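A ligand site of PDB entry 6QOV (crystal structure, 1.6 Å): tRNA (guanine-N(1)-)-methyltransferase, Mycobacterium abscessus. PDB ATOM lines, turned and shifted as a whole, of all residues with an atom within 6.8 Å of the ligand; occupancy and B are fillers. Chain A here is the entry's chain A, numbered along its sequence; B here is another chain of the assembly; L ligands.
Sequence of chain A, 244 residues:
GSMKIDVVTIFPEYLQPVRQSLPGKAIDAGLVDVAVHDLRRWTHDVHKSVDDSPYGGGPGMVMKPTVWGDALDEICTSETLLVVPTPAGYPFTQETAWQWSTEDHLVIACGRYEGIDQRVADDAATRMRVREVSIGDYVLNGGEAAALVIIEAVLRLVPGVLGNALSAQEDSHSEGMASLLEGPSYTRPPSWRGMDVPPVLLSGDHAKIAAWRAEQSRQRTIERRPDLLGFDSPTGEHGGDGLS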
ATOM      1  N   VAL A  84      11.971 -25.264 -28.223  1.00  0.00           N
ATOM      2  CA  VAL A  84      13.135 -25.151 -27.326  1.00  0.00           C
ATOM      3  C   VAL A  84      14.321 -25.971 -27.860  1.00  0.00           C
ATOM      4  O   VAL A  84      14.337 -27.207 -27.694  1.00  0.00           O
ATOM      5  CB  VAL A  84      12.807 -25.626 -25.885  1.00  0.00           C
ATOM      6  CG1 VAL A  84      13.982 -25.317 -24.965  1.00  0.00           C
ATOM      7  CG2 VAL A  84      11.522 -24.971 -25.366  1.00  0.00           C
ATOM      8  N   PRO A  85      15.320 -25.320 -28.498  1.00  0.00           N
ATOM      9  CA  PRO A  85      16.467 -26.106 -28.968  1.00  0.00           C
ATOM     10  C   PRO A  85      17.342 -26.618 -27.818  1.00  0.00           C
ATOM     11  O   PRO A  85      17.713 -25.863 -26.908  1.00  0.00           O
ATOM     12  CB  PRO A  85      17.246 -25.131 -29.853  1.00  0.00           C
ATOM     13  CG  PRO A  85      16.234 -24.034 -30.243  1.00  0.00           C
ATOM     14  CD  PRO A  85      15.333 -23.942 -29.013  1.00  0.00           C
ATOM     15  N   THR A  86      17.677 -27.911 -27.869  1.00  0.00           N
ATOM     16  CA  THR A  86      18.453 -28.557 -26.817  1.00  0.00           C
ATOM     17  C   THR A  86      19.065 -29.856 -27.366  1.00  0.00           C
ATOM     18  O   THR A  86      18.398 -30.536 -28.140  1.00  0.00           O
ATOM     19  CB  THR A  86      17.591 -28.863 -25.556  1.00  0.00           C
ATOM     20  OG1 THR A  86      18.260 -29.830 -24.741  1.00  0.00           O
ATOM     21  CG2 THR A  86      16.195 -29.389 -25.924  1.00  0.00           C
ATOM     22  N   PRO A  87      20.298 -30.174 -26.964  1.00  0.00           N
ATOM     23  CA  PRO A  87      20.902 -31.425 -27.464  1.00  0.00           C
ATOM     24  C   PRO A  87      20.194 -32.654 -26.922  1.00  0.00           C
ATOM     25  O   PRO A  87      20.415 -33.760 -27.453  1.00  0.00           O
ATOM     26  CB  PRO A  87      22.357 -31.349 -26.986  1.00  0.00           C
ATOM     27  CG  PRO A  87      22.325 -30.444 -25.787  1.00  0.00           C
ATOM     28  CD  PRO A  87      21.204 -29.449 -26.051  1.00  0.00           C
ATOM     29  N   ALA A  88      19.320 -32.477 -25.927  1.00  0.00           N
ATOM     30  CA  ALA A  88      18.525 -33.576 -25.393  1.00  0.00           C
ATOM     31  C   ALA A  88      17.123 -33.672 -25.997  1.00  0.00           C
ATOM     32  O   ALA A  88      16.257 -34.368 -25.466  1.00  0.00           O
ATOM     33  CB  ALA A  88      18.421 -33.450 -23.860  1.00  0.00           C
ATOM     34  N   CYS A 110      15.799 -19.588 -26.618  1.00  0.00           N
ATOM     35  CA  CYS A 110      17.227 -19.928 -26.698  1.00  0.00           C
ATOM     36  C   CYS A 110      17.900 -19.944 -25.337  1.00  0.00           C
ATOM     37  O   CYS A 110      18.034 -18.906 -24.687  1.00  0.00           O
ATOM     38  CB  CYS A 110      17.980 -18.945 -27.602  1.00  0.00           C
ATOM     39  SG  CYS A 110      17.419 -18.865 -29.335  1.00  0.00           S
ATOM     40  N   GLY A 111      18.358 -21.131 -24.932  1.00  0.00           N
ATOM     41  CA  GLY A 111      19.092 -21.280 -23.687  1.00  0.00           C
ATOM     42  C   GLY A 111      20.587 -21.032 -23.803  1.00  0.00           C
ATOM     43  O   GLY A 111      21.147 -21.033 -24.907  1.00  0.00           O
ATOM     44  N   ARG A 112      21.215 -20.809 -22.644  1.00  0.00           N
ATOM     45  CA  ARG A 112      22.674 -20.690 -22.497  1.00  0.00           C
ATOM     46  C   ARG A 112      23.039 -21.432 -21.203  1.00  0.00           C
ATOM     47  O   ARG A 112      22.161 -22.051 -20.590  1.00  0.00           O
ATOM     48  CB  ARG A 112      23.123 -19.213 -22.453  1.00  0.00           C
ATOM     49  CG  ARG A 112      23.133 -18.527 -23.827  1.00  0.00           C
ATOM     50  CD  ARG A 112      24.527 -18.573 -24.455  1.00  0.00           C
ATOM     51  NE  ARG A 112      24.488 -18.517 -25.913  1.00  0.00           N
ATOM     52  CZ  ARG A 112      25.556 -18.390 -26.684  1.00  0.00           C
ATOM     53  NH1 ARG A 112      26.766 -18.250 -26.138  1.00  0.00           N
ATOM     54  NH2 ARG A 112      25.430 -18.351 -28.007  1.00  0.00           N
ATOM     55  N   TYR A 113      24.301 -21.367 -20.799  1.00  0.00           N
ATOM     56  CA  TYR A 113      24.782 -22.090 -19.611  1.00  0.00           C
ATOM     57  C   TYR A 113      24.435 -23.574 -19.747  1.00  0.00           C
ATOM     58  O   TYR A 113      24.642 -24.168 -20.808  1.00  0.00           O
ATOM     59  CB  TYR A 113      24.181 -21.495 -18.331  1.00  0.00           C
ATOM     60  CG  TYR A 113      24.359 -19.986 -18.189  1.00  0.00           C
ATOM     61  CD1 TYR A 113      23.403 -19.112 -18.673  1.00  0.00           C
ATOM     62  CD2 TYR A 113      25.492 -19.457 -17.578  1.00  0.00           C
ATOM     63  CE1 TYR A 113      23.561 -17.737 -18.563  1.00  0.00           C
ATOM     64  CE2 TYR A 113      25.659 -18.093 -17.460  1.00  0.00           C
ATOM     65  CZ  TYR A 113      24.696 -17.235 -17.946  1.00  0.00           C
ATOM     66  OH  TYR A 113      24.852 -15.880 -17.826  1.00  0.00           O
ATOM     67  N   GLU A 114      23.891 -24.192 -18.700  1.00  0.00           N
ATOM     68  CA  GLU A 114      23.510 -25.603 -18.796  1.00  0.00           C
ATOM     69  C   GLU A 114      22.027 -25.834 -19.123  1.00  0.00           C
ATOM     70  O   GLU A 114      21.518 -26.940 -18.919  1.00  0.00           O
ATOM     71  CB  GLU A 114      23.877 -26.322 -17.495  1.00  0.00           C
ATOM     72  CG  GLU A 114      25.365 -26.274 -17.146  1.00  0.00           C
ATOM     73  CD  GLU A 114      26.285 -26.455 -18.354  1.00  0.00           C
ATOM     74  OE1 GLU A 114      27.126 -25.575 -18.603  1.00  0.00           O
ATOM     75  OE2 GLU A 114      26.158 -27.490 -19.052  1.00  0.00           O
ATOM     76  N   GLY A 115      21.335 -24.825 -19.645  1.00  0.00           N
ATOM     77  CA  GLY A 115      19.947 -24.964 -20.073  1.00  0.00           C
ATOM     78  C   GLY A 115      18.943 -24.265 -19.165  1.00  0.00           C
ATOM     79  O   GLY A 115      19.344 -23.520 -18.276  1.00  0.00           O
ATOM     80  N   ILE A 116      17.656 -24.508 -19.394  1.00  0.00           N
ATOM     81  CA  ILE A 116      16.558 -23.803 -18.731  1.00  0.00           C
ATOM     82  C   ILE A 116      15.863 -24.714 -17.702  1.00  0.00           C
ATOM     83  O   ILE A 116      15.612 -25.881 -18.005  1.00  0.00           O
ATOM     84  CB  ILE A 116      15.510 -23.298 -19.767  1.00  0.00           C
ATOM     85  CG1 ILE A 116      16.185 -22.464 -20.867  1.00  0.00           C
ATOM     86  CG2 ILE A 116      14.366 -22.514 -19.065  1.00  0.00           C
ATOM     87  CD1 ILE A 116      15.282 -22.070 -22.042  1.00  0.00           C
ATOM     88  N   VAL A 133      13.688 -29.826 -29.182  1.00  0.00           N
ATOM     89  CA  VAL A 133      14.312 -30.484 -30.363  1.00  0.00           C
ATOM     90  C   VAL A 133      15.811 -30.244 -30.483  1.00  0.00           C
ATOM     91  O   VAL A 133      16.312 -29.185 -30.075  1.00  0.00           O
ATOM     92  CB  VAL A 133      13.666 -30.003 -31.713  1.00  0.00           C
ATOM     93  CG1 VAL A 133      12.197 -30.422 -31.828  1.00  0.00           C
ATOM     94  CG2 VAL A 133      13.826 -28.502 -31.925  1.00  0.00           C
ATOM     95  N   SER A 134      16.491 -31.209 -31.089  1.00  0.00           N
ATOM     96  CA  SER A 134      17.912 -31.122 -31.422  1.00  0.00           C
ATOM     97  C   SER A 134      18.096 -31.107 -32.941  1.00  0.00           C
ATOM     98  O   SER A 134      17.420 -31.860 -33.656  1.00  0.00           O
ATOM     99  CB  SER A 134      18.688 -32.305 -30.833  1.00  0.00           C
ATOM    100  OG  SER A 134      20.002 -32.365 -31.374  1.00  0.00           O
ATOM    101  N   ILE A 135      19.023 -30.285 -33.425  1.00  0.00           N
ATOM    102  CA  ILE A 135      19.317 -30.235 -34.863  1.00  0.00           C
ATOM    103  C   ILE A 135      20.449 -31.193 -35.285  1.00  0.00           C
ATOM    104  O   ILE A 135      20.748 -31.325 -36.482  1.00  0.00           O
ATOM    105  CB  ILE A 135      19.678 -28.790 -35.334  1.00  0.00           C
ATOM    106  CG1 ILE A 135      20.923 -28.252 -34.636  1.00  0.00           C
ATOM    107  CG2 ILE A 135      18.465 -27.842 -35.136  1.00  0.00           C
ATOM    108  CD1 ILE A 135      21.590 -27.083 -35.408  1.00  0.00           C
ATOM    109  N   GLY A 136      21.091 -31.863 -34.317  1.00  0.00           N
ATOM    110  CA  GLY A 136      22.147 -32.816 -34.610  1.00  0.00           C
ATOM    111  C   GLY A 136      22.873 -33.232 -33.347  1.00  0.00           C
ATOM    112  O   GLY A 136      22.669 -32.632 -32.294  1.00  0.00           O
ATOM    113  N   ASP A 137      23.713 -34.262 -33.437  1.00  0.00           N
ATOM    114  CA  ASP A 137      24.338 -34.823 -32.229  1.00  0.00           C
ATOM    115  C   ASP A 137      25.661 -34.145 -31.844  1.00  0.00           C
ATOM    116  O   ASP A 137      26.728 -34.716 -31.981  1.00  0.00           O
ATOM    117  CB  ASP A 137      24.539 -36.315 -32.392  1.00  0.00           C
ATOM    118  CG  ASP A 137      23.237 -37.089 -32.337  1.00  0.00           C
ATOM    119  OD1 ASP A 137      22.251 -36.531 -31.804  1.00  0.00           O
ATOM    120  OD2 ASP A 137      23.212 -38.233 -32.800  1.00  0.00           O
ATOM    121  N   TYR A 138      25.545 -32.909 -31.351  1.00  0.00           N
ATOM    122  CA  TYR A 138      26.690 -32.122 -30.886  1.00  0.00           C
ATOM    123  C   TYR A 138      26.186 -31.082 -29.876  1.00  0.00           C
ATOM    124  O   TYR A 138      25.005 -30.717 -29.862  1.00  0.00           O
ATOM    125  CB  TYR A 138      27.424 -31.451 -32.071  1.00  0.00           C
ATOM    126  CG  TYR A 138      26.467 -31.018 -33.160  1.00  0.00           C
ATOM    127  CD1 TYR A 138      25.684 -29.867 -33.016  1.00  0.00           C
ATOM    128  CD2 TYR A 138      26.324 -31.766 -34.321  1.00  0.00           C
ATOM    129  CE1 TYR A 138      24.774 -29.490 -33.991  1.00  0.00           C
ATOM    130  CE2 TYR A 138      25.430 -31.393 -35.318  1.00  0.00           C
ATOM    131  CZ  TYR A 138      24.656 -30.250 -35.148  1.00  0.00           C
ATOM    132  OH  TYR A 138      23.724 -29.843 -36.082  1.00  0.00           O
ATOM    133  N   VAL A 139      27.104 -30.634 -29.026  1.00  0.00           N
ATOM    134  CA  VAL A 139      26.799 -29.611 -28.030  1.00  0.00           C
ATOM    135  C   VAL A 139      27.302 -28.266 -28.512  1.00  0.00           C
ATOM    136  O   VAL A 139      28.426 -28.166 -28.991  1.00  0.00           O
ATOM    137  CB  VAL A 139      27.422 -29.950 -26.661  1.00  0.00           C
ATOM    138  CG1 VAL A 139      27.273 -28.783 -25.693  1.00  0.00           C
ATOM    139  CG2 VAL A 139      26.770 -31.206 -26.100  1.00  0.00           C
ATOM    140  N   LEU A 140      26.462 -27.232 -28.405  1.00  0.00           N
ATOM    141  CA  LEU A 140      26.855 -25.852 -28.736  1.00  0.00           C
ATOM    142  C   LEU A 140      27.048 -25.030 -27.438  1.00  0.00           C
ATOM    143  O   LEU A 140      26.949 -25.569 -26.332  1.00  0.00           O
ATOM    144  CB  LEU A 140      25.787 -25.208 -29.645  1.00  0.00           C
ATOM    145  CG  LEU A 140      25.495 -25.972 -30.945  1.00  0.00           C
ATOM    146  CD1 LEU A 140      24.277 -25.420 -31.671  1.00  0.00           C
ATOM    147  CD2 LEU A 140      26.713 -25.968 -31.876  1.00  0.00           C
ATOM    148  N   ASN A 141      27.323 -23.737 -27.582  1.00  0.00           N
ATOM    149  CA  ASN A 141      27.380 -22.864 -26.392  1.00  0.00           C
ATOM    150  C   ASN A 141      26.002 -22.360 -25.955  1.00  0.00           C
ATOM    151  O   ASN A 141      25.834 -21.896 -24.815  1.00  0.00           O
ATOM    152  CB  ASN A 141      28.295 -21.673 -26.646  1.00  0.00           C
ATOM    153  CG  ASN A 141      29.768 -22.037 -26.600  1.00  0.00           C
ATOM    154  OD1 ASN A 141      30.185 -22.854 -25.775  1.00  0.00           O
ATOM    155  ND2 ASN A 141      30.550 -21.441 -27.482  1.00  0.00           N
ATOM    156  N   GLY A 142      25.037 -22.452 -26.862  1.00  0.00           N
ATOM    157  CA  GLY A 142      23.688 -21.986 -26.617  1.00  0.00           C
ATOM    158  C   GLY A 142      22.755 -22.340 -27.769  1.00  0.00           C
ATOM    159  O   GLY A 142      23.192 -22.917 -28.774  1.00  0.00           O
ATOM    160  N   GLY A 143      21.483 -21.989 -27.633  1.00  0.00           N
ATOM    161  CA  GLY A 143      20.511 -22.343 -28.654  1.00  0.00           C
ATOM    162  C   GLY A 143      20.446 -21.449 -29.901  1.00  0.00           C
ATOM    163  O   GLY A 143      19.733 -21.803 -30.851  1.00  0.00           O
ATOM    164  N   GLU A 144      21.153 -20.320 -29.896  1.00  0.00           N
ATOM    165  CA  GLU A 144      21.043 -19.332 -30.983  1.00  0.00           C
ATOM    166  C   GLU A 144      21.411 -19.888 -32.385  1.00  0.00           C
ATOM    167  O   GLU A 144      20.666 -19.657 -33.353  1.00  0.00           O
ATOM    168  CB  GLU A 144      21.912 -18.114 -30.666  1.00  0.00           C
ATOM    169  CG  GLU A 144      21.346 -17.246 -29.537  1.00  0.00           C
ATOM    170  CD  GLU A 144      21.675 -17.752 -28.128  1.00  0.00           C
ATOM    171  OE1 GLU A 144      22.425 -18.734 -27.993  1.00  0.00           O
ATOM    172  OE2 GLU A 144      21.170 -17.145 -27.161  1.00  0.00           O
ATOM    173  N   ALA A 146      21.306 -22.966 -33.385  1.00  0.00           N
ATOM    174  CA  ALA A 146      20.250 -23.923 -33.737  1.00  0.00           C
ATOM    175  C   ALA A 146      18.974 -23.204 -34.183  1.00  0.00           C
ATOM    176  O   ALA A 146      18.308 -23.642 -35.136  1.00  0.00           O
ATOM    177  CB  ALA A 146      19.956 -24.862 -32.562  1.00  0.00           C
ATOM    178  N   ILE A 150      16.913 -23.751 -37.734  1.00  0.00           N
ATOM    179  CA  ILE A 150      15.458 -24.012 -37.745  1.00  0.00           C
ATOM    180  C   ILE A 150      14.672 -22.955 -38.547  1.00  0.00           C
ATOM    181  O   ILE A 150      13.800 -23.298 -39.375  1.00  0.00           O
ATOM    182  CB  ILE A 150      14.922 -24.108 -36.297  1.00  0.00           C
ATOM    183  CG1 ILE A 150      15.456 -25.384 -35.626  1.00  0.00           C
ATOM    184  CG2 ILE A 150      13.370 -24.103 -36.296  1.00  0.00           C
ATOM    185  CD1 ILE A 150      15.336 -25.373 -34.084  1.00  0.00           C
ATOM    186  N   GLU B 152      31.044 -23.109 -33.943  1.00  0.00           N
ATOM    187  CA  GLU B 152      30.742 -23.097 -32.514  1.00  0.00           C
ATOM    188  C   GLU B 152      31.047 -24.442 -31.845  1.00  0.00           C
ATOM    189  O   GLU B 152      31.635 -24.473 -30.755  1.00  0.00           O
ATOM    190  CB  GLU B 152      29.282 -22.737 -32.285  1.00  0.00           C
ATOM    191  CG  GLU B 152      28.939 -22.565 -30.818  1.00  0.00           C
ATOM    192  CD  GLU B 152      27.678 -21.732 -30.598  1.00  0.00           C
ATOM    193  OE1 GLU B 152      27.318 -20.922 -31.469  1.00  0.00           O
ATOM    194  OE2 GLU B 152      27.061 -21.912 -29.527  1.00  0.00           O
HETATM  195  C1  LIG L   1      21.366 -25.135 -25.508  1.00  0.00           C
HETATM  196  C2  LIG L   1      23.938 -24.887 -24.504  1.00  0.00           C
HETATM  197  N1  LIG L   1      20.422 -28.888 -31.350  1.00  0.00           N
HETATM  198  C3  LIG L   1      21.748 -28.887 -30.871  1.00  0.00           C
HETATM  199  C4  LIG L   1      21.867 -27.975 -29.661  1.00  0.00           C
HETATM  200  C5  LIG L   1      20.828 -27.126 -29.266  1.00  0.00           C
HETATM  201  C6  LIG L   1      21.011 -26.316 -28.132  1.00  0.00           C
HETATM  202  C7  LIG L   1      22.212 -26.355 -27.418  1.00  0.00           C
HETATM  203  N2  LIG L   1      23.185 -27.202 -27.844  1.00  0.00           N
HETATM  204  C8  LIG L   1      23.038 -27.990 -28.929  1.00  0.00           C
HETATM  205  C9  LIG L   1      22.440 -25.641 -26.243  1.00  0.00           C
HETATM  206  C10 LIG L   1      21.593 -24.463 -24.298  1.00  0.00           C
HETATM  207  C11 LIG L   1      22.874 -24.350 -23.794  1.00  0.00           C
HETATM  208  C12 LIG L   1      23.718 -25.543 -25.711  1.00  0.00           C
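The backbone NH of Leu 140 sits at hydrogen-bond distance from a nitrogen (N2) of the ligand. N1 of the ligand sits close to N of Ile 135 (2.9 Å).
The backbone NH of Thr 86 is in hydrogen-bond range of the backbone carbonyl oxygen of Val 133. N of Ala 88 sits close to OG1 of Thr 86 (3.1 Å). The side-chain hydroxyl (OG) of Ser 134 sits at hydrogen-bond distance from the backbone carbonyl oxygen (O) of Gly 136, 2.8 Å away. N of Gly 143 lies within hydrogen-bond range of O of Gly 111. The side-chain carboxylate of Glu 152 of chain B is in hydrogen-bond range of the backbone NH of Asn 141 (2.7 Å). The guanidinium group (NE) of Arg 112 lies within salt-bridge range of the side-chain carboxylate (OE1) of Glu 144, at 2.9 Å. N of Gly 142 lies within hydrogen-bond range of OE2 of Glu 152 of chain B (3.4 Å). O of Ile 135 is in hydrogen-bond range of OH of Tyr 138, 3.3 Å away.
Merely in contact with the ligand: Ser 134 (3.4 Å), Tyr 113 (3.5 Å), Tyr 138 (3.5 Å), Pro 87 (3.5 Å), Gly 111 (3.5 Å), Thr 86 (3.5 Å), Pro 85 (3.5 Å), Gly 142 (3.6 Å), Asn 141 (3.6 Å), Gly 143 (3.8 Å) and Arg 112 (3.9 Å). Hydrophobic or aromatic side chains within 4 Å of the ligand: Pro 87, Ile 135 and Leu 140. Within 4 Å of the ligand: Pro 85, Thr 86, Pro 87, Gly 111, Arg 112, Tyr 113, Ser 134, Ile 135, Tyr 138, Leu 140, Asn 141, Gly 142 and Gly 143.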
